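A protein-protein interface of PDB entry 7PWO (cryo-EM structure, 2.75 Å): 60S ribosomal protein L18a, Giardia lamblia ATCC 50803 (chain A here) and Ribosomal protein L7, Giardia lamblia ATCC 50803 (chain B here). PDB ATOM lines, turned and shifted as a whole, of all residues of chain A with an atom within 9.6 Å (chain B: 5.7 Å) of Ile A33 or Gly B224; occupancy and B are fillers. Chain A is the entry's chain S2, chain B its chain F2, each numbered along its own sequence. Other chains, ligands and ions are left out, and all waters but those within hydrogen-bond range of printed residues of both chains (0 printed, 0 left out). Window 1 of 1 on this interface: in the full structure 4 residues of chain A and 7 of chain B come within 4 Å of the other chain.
Of the 11 printed residues of chain B, 5 touch a printed residue of chain A.
Hydrophobic or aromatic side chains of chain B that line the printed part of chain A: Tyr B226.
Of the 22 printed residues of chain A, 3 touch a printed residue of chain B.
Hydrophobic or aromatic side chains of chain A that line the printed part of chain B: Ile A33 and His A116.
The backbone carbonyl oxygen (O) of Gly B224 is in hydrogen-bond range of the backbone NH (N) of Glu B133 (3.3 Å).
The guanidinium group of Arg A38 is in hydrogen-bond range of a ring nitrogen (ND1) of His A116, 2.9 Å away.
The side-chain amide oxygen of Asn A31 sits at hydrogen-bond distance from the backbone NH of Ile A33.
The backbone carbonyl oxygen (O) of Tyr B131 is in hydrogen-bond range of the backbone NH (N) of Arg B223 (3.1 Å).
NE2 of His A116 sits at hydrogen-bond distance from O of Ala B215 (3.4 Å).
Of the printed residues of chain B, Asn A31 touches Tyr B226.
Ile A33 touches just these residues of chain B: Tyr B222, Arg B223 and Gly B224.
No residue of chain A comes within 4 Å of Glu B133.
Of the printed residues of chain A, Tyr B222 touches Ile A33 (3.9 Å).
Gly B224 touches just one residue of chain A: Ile A33.
The nearest residue of chain B that does not touch Ile A33 is Phe B214 (4.1 Å).
The nearest printed residue of chain B that does not touch His A116 is Phe B214 (7.3 Å).
Asn A31 touches Tyr B226.
Ile A33 touches Tyr B222.
CG1 of Ile A33 touches O of Arg B223, at 3.9 Å.
CA of Gly B224 touches CD1 of Ile A33, at 3.9 Å.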
ATOM      1  N   GLN A   3     -13.768 -20.381   5.773  1.00  0.00           N
ATOM      2  CA  GLN A   3     -13.909 -19.579   6.966  1.00  0.00           C
ATOM      3  C   GLN A   3     -14.326 -20.498   8.100  1.00  0.00           C
ATOM      4  O   GLN A   3     -14.940 -21.548   7.875  1.00  0.00           O
ATOM      5  CB  GLN A   3     -14.930 -18.458   6.746  1.00  0.00           C
ATOM      6  CG  GLN A   3     -14.612 -17.607   5.521  1.00  0.00           C
ATOM      7  CD  GLN A   3     -15.430 -16.341   5.440  1.00  0.00           C
ATOM      8  OE1 GLN A   3     -15.257 -15.426   6.241  1.00  0.00           O
ATOM      9  NE2 GLN A   3     -16.339 -16.285   4.482  1.00  0.00           N
ATOM     10  N   TYR A   5     -16.384 -21.268  11.482  1.00  0.00           N
ATOM     11  CA  TYR A   5     -17.607 -20.939  12.192  1.00  0.00           C
ATOM     12  C   TYR A   5     -17.786 -21.908  13.354  1.00  0.00           C
ATOM     13  O   TYR A   5     -17.439 -23.081  13.245  1.00  0.00           O
ATOM     14  CB  TYR A   5     -18.836 -21.013  11.270  1.00  0.00           C
ATOM     15  CG  TYR A   5     -18.837 -20.075  10.081  1.00  0.00           C
ATOM     16  CD1 TYR A   5     -18.239 -20.436   8.879  1.00  0.00           C
ATOM     17  CD2 TYR A   5     -19.388 -18.818  10.177  1.00  0.00           C
ATOM     18  CE1 TYR A   5     -18.245 -19.586   7.806  1.00  0.00           C
ATOM     19  CE2 TYR A   5     -19.395 -17.965   9.116  1.00  0.00           C
ATOM     20  CZ  TYR A   5     -18.820 -18.343   7.934  1.00  0.00           C
ATOM     21  OH  TYR A   5     -18.822 -17.460   6.875  1.00  0.00           O
ATOM     22  N   VAL A   7     -21.028 -23.263  15.498  1.00  0.00           N
ATOM     23  CA  VAL A   7     -22.481 -23.242  15.444  1.00  0.00           C
ATOM     24  C   VAL A   7     -23.021 -23.939  16.683  1.00  0.00           C
ATOM     25  O   VAL A   7     -22.602 -25.059  17.005  1.00  0.00           O
ATOM     26  CB  VAL A   7     -23.016 -23.900  14.164  1.00  0.00           C
ATOM     27  CG1 VAL A   7     -24.513 -23.931  14.197  1.00  0.00           C
ATOM     28  CG2 VAL A   7     -22.518 -23.184  12.950  1.00  0.00           C
ATOM     29  N   ILE A  27     -17.172 -25.666  12.166  1.00  0.00           N
ATOM     30  CA  ILE A  27     -17.481 -25.889  10.760  1.00  0.00           C
ATOM     31  C   ILE A  27     -16.521 -25.057   9.922  1.00  0.00           C
ATOM     32  O   ILE A  27     -16.227 -23.907  10.260  1.00  0.00           O
ATOM     33  CB  ILE A  27     -18.946 -25.518  10.433  1.00  0.00           C
ATOM     34  CG1 ILE A  27     -19.931 -26.331  11.277  1.00  0.00           C
ATOM     35  CG2 ILE A  27     -19.251 -25.736   8.966  1.00  0.00           C
ATOM     36  CD1 ILE A  27     -19.853 -27.791  11.071  1.00  0.00           C
ATOM     37  N   ALA A  29     -16.410 -23.622   6.236  1.00  0.00           N
ATOM     38  CA  ALA A  29     -17.364 -23.460   5.150  1.00  0.00           C
ATOM     39  C   ALA A  29     -17.010 -22.233   4.333  1.00  0.00           C
ATOM     40  O   ALA A  29     -16.319 -21.334   4.819  1.00  0.00           O
ATOM     41  CB  ALA A  29     -18.799 -23.345   5.675  1.00  0.00           C
ATOM     42  N   PRO A  30     -17.433 -22.187   3.068  1.00  0.00           N
ATOM     43  CA  PRO A  30     -17.306 -20.932   2.314  1.00  0.00           C
ATOM     44  C   PRO A  30     -18.102 -19.777   2.894  1.00  0.00           C
ATOM     45  O   PRO A  30     -17.631 -18.637   2.808  1.00  0.00           O
ATOM     46  CB  PRO A  30     -17.789 -21.306   0.907  1.00  0.00           C
ATOM     47  CG  PRO A  30     -18.377 -22.655   1.013  1.00  0.00           C
ATOM     48  CD  PRO A  30     -17.796 -23.320   2.204  1.00  0.00           C
ATOM     49  N   ASN A  31     -19.285 -20.010   3.466  1.00  0.00           N
ATOM     50  CA  ASN A  31     -20.052 -18.936   4.093  1.00  0.00           C
ATOM     51  C   ASN A  31     -21.113 -19.522   5.025  1.00  0.00           C
ATOM     52  O   ASN A  31     -21.205 -20.739   5.223  1.00  0.00           O
ATOM     53  CB  ASN A  31     -20.673 -17.993   3.054  1.00  0.00           C
ATOM     54  CG  ASN A  31     -21.638 -18.688   2.110  1.00  0.00           C
ATOM     55  OD1 ASN A  31     -22.714 -19.119   2.506  1.00  0.00           O
ATOM     56  ND2 ASN A  31     -21.267 -18.756   0.838  1.00  0.00           N
ATOM     57  N   GLU A  32     -21.920 -18.613   5.596  1.00  0.00           N
ATOM     58  CA  GLU A  32     -22.800 -18.921   6.721  1.00  0.00           C
ATOM     59  C   GLU A  32     -23.908 -19.892   6.339  1.00  0.00           C
ATOM     60  O   GLU A  32     -24.273 -20.774   7.127  1.00  0.00           O
ATOM     61  CB  GLU A  32     -23.405 -17.630   7.267  1.00  0.00           C
ATOM     62  CG  GLU A  32     -24.001 -17.787   8.649  1.00  0.00           C
ATOM     63  CD  GLU A  32     -25.147 -16.839   8.941  1.00  0.00           C
ATOM     64  OE1 GLU A  32     -26.075 -16.744   8.117  1.00  0.00           O
ATOM     65  OE2 GLU A  32     -25.129 -16.200  10.015  1.00  0.00           O
ATOM     66  N   ILE A  33     -24.466 -19.738   5.140  1.00  0.00           N
ATOM     67  CA  ILE A  33     -25.567 -20.596   4.715  1.00  0.00           C
ATOM     68  C   ILE A  33     -25.093 -22.045   4.584  1.00  0.00           C
ATOM     69  O   ILE A  33     -25.723 -22.974   5.110  1.00  0.00           O
ATOM     70  CB  ILE A  33     -26.167 -20.047   3.406  1.00  0.00           C
ATOM     71  CG1 ILE A  33     -26.408 -18.543   3.547  1.00  0.00           C
ATOM     72  CG2 ILE A  33     -27.470 -20.708   3.073  1.00  0.00           C
ATOM     73  CD1 ILE A  33     -27.354 -18.139   4.667  1.00  0.00           C
ATOM     74  N   VAL A  34     -23.944 -22.254   3.941  1.00  0.00           N
ATOM     75  CA  VAL A  34     -23.388 -23.603   3.839  1.00  0.00           C
ATOM     76  C   VAL A  34     -23.015 -24.140   5.216  1.00  0.00           C
ATOM     77  O   VAL A  34     -23.187 -25.329   5.501  1.00  0.00           O
ATOM     78  CB  VAL A  34     -22.181 -23.622   2.887  1.00  0.00           C
ATOM     79  CG1 VAL A  34     -21.666 -25.051   2.712  1.00  0.00           C
ATOM     80  CG2 VAL A  34     -22.553 -23.016   1.557  1.00  0.00           C
ATOM     81  N   ALA A  35     -22.506 -23.272   6.093  1.00  0.00           N
ATOM     82  CA  ALA A  35     -22.110 -23.723   7.424  1.00  0.00           C
ATOM     83  C   ALA A  35     -23.303 -24.251   8.216  1.00  0.00           C
ATOM     84  O   ALA A  35     -23.232 -25.330   8.817  1.00  0.00           O
ATOM     85  CB  ALA A  35     -21.410 -22.588   8.171  1.00  0.00           C
ATOM     86  N   LYS A  36     -24.418 -23.513   8.224  1.00  0.00           N
ATOM     87  CA  LYS A  36     -25.587 -23.999   8.957  1.00  0.00           C
ATOM     88  C   LYS A  36     -26.177 -25.243   8.317  1.00  0.00           C
ATOM     89  O   LYS A  36     -26.651 -26.138   9.027  1.00  0.00           O
ATOM     90  CB  LYS A  36     -26.675 -22.937   9.069  1.00  0.00           C
ATOM     91  CG  LYS A  36     -26.294 -21.726   9.848  1.00  0.00           C
ATOM     92  CD  LYS A  36     -27.464 -20.784   9.957  1.00  0.00           C
ATOM     93  CE  LYS A  36     -27.762 -20.171   8.611  1.00  0.00           C
ATOM     94  NZ  LYS A  36     -26.686 -19.307   8.136  1.00  0.00           N
ATOM     95  N   SER A  37     -26.153 -25.323   6.985  1.00  0.00           N
ATOM     96  CA  SER A  37     -26.629 -26.531   6.321  1.00  0.00           C
ATOM     97  C   SER A  37     -25.818 -27.752   6.746  1.00  0.00           C
ATOM     98  O   SER A  37     -26.375 -28.832   6.978  1.00  0.00           O
ATOM     99  CB  SER A  37     -26.575 -26.331   4.808  1.00  0.00           C
ATOM    100  OG  SER A  37     -26.992 -27.477   4.107  1.00  0.00           O
ATOM    101  N   ARG A  38     -24.500 -27.598   6.858  1.00  0.00           N
ATOM    102  CA  ARG A  38     -23.645 -28.717   7.248  1.00  0.00           C
ATOM    103  C   ARG A  38     -23.810 -29.077   8.724  1.00  0.00           C
ATOM    104  O   ARG A  38     -23.746 -30.263   9.093  1.00  0.00           O
ATOM    105  CB  ARG A  38     -22.199 -28.373   6.913  1.00  0.00           C
ATOM    106  CG  ARG A  38     -21.204 -29.432   7.286  1.00  0.00           C
ATOM    107  CD  ARG A  38     -21.377 -30.719   6.486  1.00  0.00           C
ATOM    108  NE  ARG A  38     -21.109 -30.586   5.057  1.00  0.00           N
ATOM    109  CZ  ARG A  38     -21.416 -31.516   4.153  1.00  0.00           C
ATOM    110  NH1 ARG A  38     -21.983 -32.654   4.523  1.00  0.00           N
ATOM    111  NH2 ARG A  38     -21.121 -31.328   2.880  1.00  0.00           N
ATOM    112  N   PHE A  39     -24.049 -28.077   9.577  1.00  0.00           N
ATOM    113  CA  PHE A  39     -24.395 -28.365  10.966  1.00  0.00           C
ATOM    114  C   PHE A  39     -25.662 -29.198  11.051  1.00  0.00           C
ATOM    115  O   PHE A  39     -25.739 -30.140  11.851  1.00  0.00           O
ATOM    116  CB  PHE A  39     -24.539 -27.062  11.759  1.00  0.00           C
ATOM    117  CG  PHE A  39     -24.983 -27.251  13.196  1.00  0.00           C
ATOM    118  CD1 PHE A  39     -26.319 -27.476  13.514  1.00  0.00           C
ATOM    119  CD2 PHE A  39     -24.057 -27.259  14.223  1.00  0.00           C
ATOM    120  CE1 PHE A  39     -26.716 -27.660  14.819  1.00  0.00           C
ATOM    121  CE2 PHE A  39     -24.455 -27.449  15.535  1.00  0.00           C
ATOM    122  CZ  PHE A  39     -25.783 -27.645  15.830  1.00  0.00           C
ATOM    123  N   TRP A  40     -26.676 -28.859  10.256  1.00  0.00           N
ATOM    124  CA  TRP A  40     -27.913 -29.633  10.307  1.00  0.00           C
ATOM    125  C   TRP A  40     -27.709 -31.036   9.757  1.00  0.00           C
ATOM    126  O   TRP A  40     -28.260 -31.996  10.297  1.00  0.00           O
ATOM    127  CB  TRP A  40     -29.034 -28.904   9.570  1.00  0.00           C
ATOM    128  CG  TRP A  40     -29.721 -27.876  10.413  1.00  0.00           C
ATOM    129  CD1 TRP A  40     -29.996 -26.595  10.064  1.00  0.00           C
ATOM    130  CD2 TRP A  40     -30.229 -28.043  11.744  1.00  0.00           C
ATOM    131  NE1 TRP A  40     -30.636 -25.953  11.081  1.00  0.00           N
ATOM    132  CE2 TRP A  40     -30.786 -26.816  12.130  1.00  0.00           C
ATOM    133  CE3 TRP A  40     -30.264 -29.110  12.645  1.00  0.00           C
ATOM    134  CZ2 TRP A  40     -31.378 -26.622  13.373  1.00  0.00           C
ATOM    135  CZ3 TRP A  40     -30.844 -28.914  13.875  1.00  0.00           C
ATOM    136  CH2 TRP A  40     -31.397 -27.684  14.227  1.00  0.00           C
ATOM    137  N   TYR A  41     -26.908 -31.175   8.699  1.00  0.00           N
ATOM    138  CA  TYR A  41     -26.470 -32.495   8.247  1.00  0.00           C
ATOM    139  C   TYR A  41     -25.976 -33.363   9.404  1.00  0.00           C
ATOM    140  O   TYR A  41     -26.485 -34.467   9.642  1.00  0.00           O
ATOM    141  CB  TYR A  41     -25.367 -32.338   7.199  1.00  0.00           C
ATOM    142  CG  TYR A  41     -24.861 -33.642   6.626  1.00  0.00           C
ATOM    143  CD1 TYR A  41     -25.497 -34.267   5.569  1.00  0.00           C
ATOM    144  CD2 TYR A  41     -23.749 -34.265   7.175  1.00  0.00           C
ATOM    145  CE1 TYR A  41     -25.024 -35.452   5.064  1.00  0.00           C
ATOM    146  CE2 TYR A  41     -23.281 -35.457   6.686  1.00  0.00           C
ATOM    147  CZ  TYR A  41     -23.917 -36.044   5.634  1.00  0.00           C
ATOM    148  OH  TYR A  41     -23.433 -37.234   5.145  1.00  0.00           O
ATOM    149  N   ARG A  51     -33.719 -30.375  10.662  1.00  0.00           N
ATOM    150  CA  ARG A  51     -33.860 -28.922  10.719  1.00  0.00           C
ATOM    151  C   ARG A  51     -35.249 -28.523  11.199  1.00  0.00           C
ATOM    152  O   ARG A  51     -35.416 -27.469  11.823  1.00  0.00           O
ATOM    153  CB  ARG A  51     -33.606 -28.306   9.342  1.00  0.00           C
ATOM    154  CG  ARG A  51     -33.753 -26.799   9.325  1.00  0.00           C
ATOM    155  CD  ARG A  51     -33.451 -26.169   7.975  1.00  0.00           C
ATOM    156  NE  ARG A  51     -32.100 -26.371   7.474  1.00  0.00           N
ATOM    157  CZ  ARG A  51     -31.727 -26.047   6.242  1.00  0.00           C
ATOM    158  NH1 ARG A  51     -32.605 -25.501   5.416  1.00  0.00           N
ATOM    159  NH2 ARG A  51     -30.486 -26.253   5.836  1.00  0.00           N
ATOM    160  N   ILE A  56     -31.177 -23.339  15.389  1.00  0.00           N
ATOM    161  CA  ILE A  56     -29.814 -22.846  15.524  1.00  0.00           C
ATOM    162  C   ILE A  56     -29.801 -21.634  16.440  1.00  0.00           C
ATOM    163  O   ILE A  56     -30.468 -20.626  16.180  1.00  0.00           O
ATOM    164  CB  ILE A  56     -29.221 -22.506  14.149  1.00  0.00           C
ATOM    165  CG1 ILE A  56     -29.121 -23.768  13.301  1.00  0.00           C
ATOM    166  CG2 ILE A  56     -27.892 -21.778  14.283  1.00  0.00           C
ATOM    167  CD1 ILE A  56     -28.798 -23.511  11.879  1.00  0.00           C
ATOM    168  N   CYS A  59     -24.333 -18.775  14.970  1.00  0.00           N
ATOM    169  CA  CYS A  59     -23.234 -19.067  14.051  1.00  0.00           C
ATOM    170  C   CYS A  59     -22.152 -18.001  14.239  1.00  0.00           C
ATOM    171  O   CYS A  59     -22.128 -16.978  13.554  1.00  0.00           O
ATOM    172  CB  CYS A  59     -23.739 -19.122  12.626  1.00  0.00           C
ATOM    173  SG  CYS A  59     -22.469 -19.067  11.371  1.00  0.00           S
ATOM    174  N   TYR A 115     -16.654 -31.470  -2.280  1.00  0.00           N
ATOM    175  CA  TYR A 115     -16.821 -30.984  -0.911  1.00  0.00           C
ATOM    176  C   TYR A 115     -17.888 -31.764  -0.145  1.00  0.00           C
ATOM    177  O   TYR A 115     -17.656 -32.177   0.994  1.00  0.00           O
ATOM    178  CB  TYR A 115     -17.144 -29.491  -0.935  1.00  0.00           C
ATOM    179  CG  TYR A 115     -17.514 -28.871   0.397  1.00  0.00           C
ATOM    180  CD1 TYR A 115     -18.812 -28.896   0.867  1.00  0.00           C
ATOM    181  CD2 TYR A 115     -16.550 -28.252   1.180  1.00  0.00           C
ATOM    182  CE1 TYR A 115     -19.140 -28.335   2.079  1.00  0.00           C
ATOM    183  CE2 TYR A 115     -16.869 -27.683   2.391  1.00  0.00           C
ATOM    184  CZ  TYR A 115     -18.164 -27.728   2.838  1.00  0.00           C
ATOM    185  OH  TYR A 115     -18.495 -27.163   4.041  1.00  0.00           O
ATOM    186  N   HIS A 116     -19.065 -31.964  -0.737  1.00  0.00           N
ATOM    187  CA  HIS A 116     -20.133 -32.689  -0.052  1.00  0.00           C
ATOM    188  C   HIS A 116     -19.910 -34.193  -0.025  1.00  0.00           C
ATOM    189  O   HIS A 116     -20.819 -34.934   0.342  1.00  0.00           O
ATOM    190  CB  HIS A 116     -21.492 -32.358  -0.676  1.00  0.00           C
ATOM    191  CG  HIS A 116     -21.911 -30.935  -0.480  1.00  0.00           C
ATOM    192  ND1 HIS A 116     -22.673 -30.519   0.590  1.00  0.00           N
ATOM    193  CD2 HIS A 116     -21.685 -29.830  -1.228  1.00  0.00           C
ATOM    194  CE1 HIS A 116     -22.901 -29.223   0.490  1.00  0.00           C
ATOM    195  NE2 HIS A 116     -22.310 -28.781  -0.604  1.00  0.00           N
ATOM    196  N   TYR B 131     -34.474 -16.266  -2.693  1.00  0.00           N
ATOM    197  CA  TYR B 131     -35.182 -15.466  -1.708  1.00  0.00           C
ATOM    198  C   TYR B 131     -34.350 -15.296  -0.448  1.00  0.00           C
ATOM    199  O   TYR B 131     -33.445 -16.078  -0.160  1.00  0.00           O
ATOM    200  CB  TYR B 131     -36.549 -16.074  -1.368  1.00  0.00           C
ATOM    201  CG  TYR B 131     -36.501 -17.471  -0.793  1.00  0.00           C
ATOM    202  CD1 TYR B 131     -36.267 -18.566  -1.602  1.00  0.00           C
ATOM    203  CD2 TYR B 131     -36.650 -17.689   0.566  1.00  0.00           C
ATOM    204  CE1 TYR B 131     -36.226 -19.826  -1.086  1.00  0.00           C
ATOM    205  CE2 TYR B 131     -36.610 -18.949   1.087  1.00  0.00           C
ATOM    206  CZ  TYR B 131     -36.392 -20.019   0.251  1.00  0.00           C
ATOM    207  OH  TYR B 131     -36.332 -21.289   0.754  1.00  0.00           O
ATOM    208  N   GLY B 132     -34.689 -14.264   0.310  1.00  0.00           N
ATOM    209  CA  GLY B 132     -34.024 -14.036   1.578  1.00  0.00           C
ATOM    210  C   GLY B 132     -34.676 -12.896   2.315  1.00  0.00           C
ATOM    211  O   GLY B 132     -35.792 -12.501   1.991  1.00  0.00           O
ATOM    212  N   GLU B 133     -33.977 -12.354   3.305  1.00  0.00           N
ATOM    213  CA  GLU B 133     -34.543 -11.284   4.103  1.00  0.00           C
ATOM    214  C   GLU B 133     -33.779  -9.975   3.915  1.00  0.00           C
ATOM    215  O   GLU B 133     -32.558  -9.933   4.107  1.00  0.00           O
ATOM    216  CB  GLU B 133     -34.613 -11.707   5.605  1.00  0.00           C
ATOM    217  CG  GLU B 133     -33.297 -11.870   6.331  1.00  0.00           C
ATOM    218  CD  GLU B 133     -32.706 -13.251   6.118  1.00  0.00           C
ATOM    219  OE1 GLU B 133     -33.158 -13.950   5.190  1.00  0.00           O
ATOM    220  OE2 GLU B 133     -31.786 -13.637   6.867  1.00  0.00           O
ATOM    221  N   PHE B 214     -28.285 -22.684  -3.609  1.00  0.00           N
ATOM    222  CA  PHE B 214     -27.247 -21.797  -3.096  1.00  0.00           C
ATOM    223  C   PHE B 214     -26.304 -22.516  -2.150  1.00  0.00           C
ATOM    224  O   PHE B 214     -25.127 -22.160  -2.069  1.00  0.00           O
ATOM    225  CB  PHE B 214     -27.871 -20.596  -2.387  1.00  0.00           C
ATOM    226  CG  PHE B 214     -26.883 -19.518  -2.053  1.00  0.00           C
ATOM    227  CD1 PHE B 214     -26.459 -18.629  -3.017  1.00  0.00           C
ATOM    228  CD2 PHE B 214     -26.368 -19.402  -0.777  1.00  0.00           C
ATOM    229  CE1 PHE B 214     -25.553 -17.648  -2.716  1.00  0.00           C
ATOM    230  CE2 PHE B 214     -25.462 -18.421  -0.477  1.00  0.00           C
ATOM    231  CZ  PHE B 214     -25.053 -17.546  -1.449  1.00  0.00           C
ATOM    232  N   ALA B 215     -26.789 -23.533  -1.443  1.00  0.00           N
ATOM    233  CA  ALA B 215     -25.953 -24.291  -0.527  1.00  0.00           C
ATOM    234  C   ALA B 215     -25.130 -25.367  -1.229  1.00  0.00           C
ATOM    235  O   ALA B 215     -24.363 -26.067  -0.565  1.00  0.00           O
ATOM    236  CB  ALA B 215     -26.813 -24.912   0.575  1.00  0.00           C
ATOM    237  N   TYR B 222     -32.903 -20.584  -0.703  1.00  0.00           N
ATOM    238  CA  TYR B 222     -32.614 -19.716   0.426  1.00  0.00           C
ATOM    239  C   TYR B 222     -31.165 -19.248   0.373  1.00  0.00           C
ATOM    240  O   TYR B 222     -30.241 -20.062   0.462  1.00  0.00           O
ATOM    241  CB  TYR B 222     -32.892 -20.489   1.711  1.00  0.00           C
ATOM    242  CG  TYR B 222     -32.803 -19.683   2.963  1.00  0.00           C
ATOM    243  CD1 TYR B 222     -33.808 -18.813   3.324  1.00  0.00           C
ATOM    244  CD2 TYR B 222     -31.707 -19.800   3.794  1.00  0.00           C
ATOM    245  CE1 TYR B 222     -33.719 -18.070   4.471  1.00  0.00           C
ATOM    246  CE2 TYR B 222     -31.608 -19.060   4.946  1.00  0.00           C
ATOM    247  CZ  TYR B 222     -32.616 -18.197   5.280  1.00  0.00           C
ATOM    248  OH  TYR B 222     -32.525 -17.460   6.430  1.00  0.00           O
ATOM    249  N   ARG B 223     -30.955 -17.941   0.234  1.00  0.00           N
ATOM    250  CA  ARG B 223     -29.607 -17.386   0.283  1.00  0.00           C
ATOM    251  C   ARG B 223     -29.410 -16.417   1.441  1.00  0.00           C
ATOM    252  O   ARG B 223     -28.359 -15.780   1.530  1.00  0.00           O
ATOM    253  CB  ARG B 223     -29.242 -16.733  -1.050  1.00  0.00           C
ATOM    254  CG  ARG B 223     -29.619 -15.286  -1.219  1.00  0.00           C
ATOM    255  CD  ARG B 223     -28.953 -14.747  -2.452  1.00  0.00           C
ATOM    256  NE  ARG B 223     -29.110 -15.654  -3.576  1.00  0.00           N
ATOM    257  CZ  ARG B 223     -28.233 -15.798  -4.563  1.00  0.00           C
ATOM    258  NH1 ARG B 223     -27.103 -15.115  -4.560  1.00  0.00           N
ATOM    259  NH2 ARG B 223     -28.479 -16.649  -5.539  1.00  0.00           N
ATOM    260  N   GLY B 224     -30.367 -16.325   2.350  1.00  0.00           N
ATOM    261  CA  GLY B 224     -30.126 -15.588   3.576  1.00  0.00           C
ATOM    262  C   GLY B 224     -30.031 -14.103   3.331  1.00  0.00           C
ATOM    263  O   GLY B 224     -30.895 -13.498   2.696  1.00  0.00           O
ATOM    264  N   LYS B 225     -28.966 -13.496   3.833  1.00  0.00           N
ATOM    265  CA  LYS B 225     -28.766 -12.059   3.738  1.00  0.00           C
ATOM    266  C   LYS B 225     -27.952 -11.652   2.515  1.00  0.00           C
ATOM    267  O   LYS B 225     -27.588 -10.483   2.390  1.00  0.00           O
ATOM    268  CB  LYS B 225     -28.105 -11.553   5.018  1.00  0.00           C
ATOM    269  CG  LYS B 225     -26.695 -12.034   5.198  1.00  0.00           C
ATOM    270  CD  LYS B 225     -26.127 -11.521   6.486  1.00  0.00           C
ATOM    271  CE  LYS B 225     -24.721 -12.019   6.695  1.00  0.00           C
ATOM    272  NZ  LYS B 225     -23.829 -11.423   5.670  1.00  0.00           N
ATOM    273  N   TYR B 226     -27.666 -12.590   1.619  1.00  0.00           N
ATOM    274  CA  TYR B 226     -26.982 -12.338   0.359  1.00  0.00           C
ATOM    275  C   TYR B 226     -27.922 -11.866  -0.747  1.00  0.00           C
ATOM    276  O   TYR B 226     -27.459 -11.525  -1.850  1.00  0.00           O
ATOM    277  CB  TYR B 226     -26.234 -13.605  -0.057  1.00  0.00           C
ATOM    278  CG  TYR B 226     -25.074 -13.904   0.872  1.00  0.00           C
ATOM    279  CD1 TYR B 226     -24.011 -13.027   0.967  1.00  0.00           C
ATOM    280  CD2 TYR B 226     -25.047 -15.049   1.655  1.00  0.00           C
ATOM    281  CE1 TYR B 226     -22.964 -13.266   1.807  1.00  0.00           C
ATOM    282  CE2 TYR B 226     -23.990 -15.303   2.503  1.00  0.00           C
ATOM    283  CZ  TYR B 226     -22.951 -14.400   2.573  1.00  0.00           C
ATOM    284  OH  TYR B 226     -21.886 -14.630   3.402  1.00  0.00           O
ATOM    285  N   ILE B 227     -29.222 -11.811  -0.467  1.00  0.00           N
ATOM    286  CA  ILE B 227     -30.175 -11.254  -1.416  1.00  0.00           C
ATOM    287  C   ILE B 227     -29.878  -9.782  -1.673  1.00  0.00           C
ATOM    288  O   ILE B 227     -30.164  -9.262  -2.759  1.00  0.00           O
ATOM    289  CB  ILE B 227     -31.615 -11.502  -0.900  1.00  0.00           C
ATOM    290  CG1 ILE B 227     -32.631 -11.395  -2.035  1.00  0.00           C
ATOM    291  CG2 ILE B 227     -31.972 -10.569   0.250  1.00  0.00           C
ATOM    292  CD1 ILE B 227     -32.648 -12.596  -2.936  1.00  0.00           C
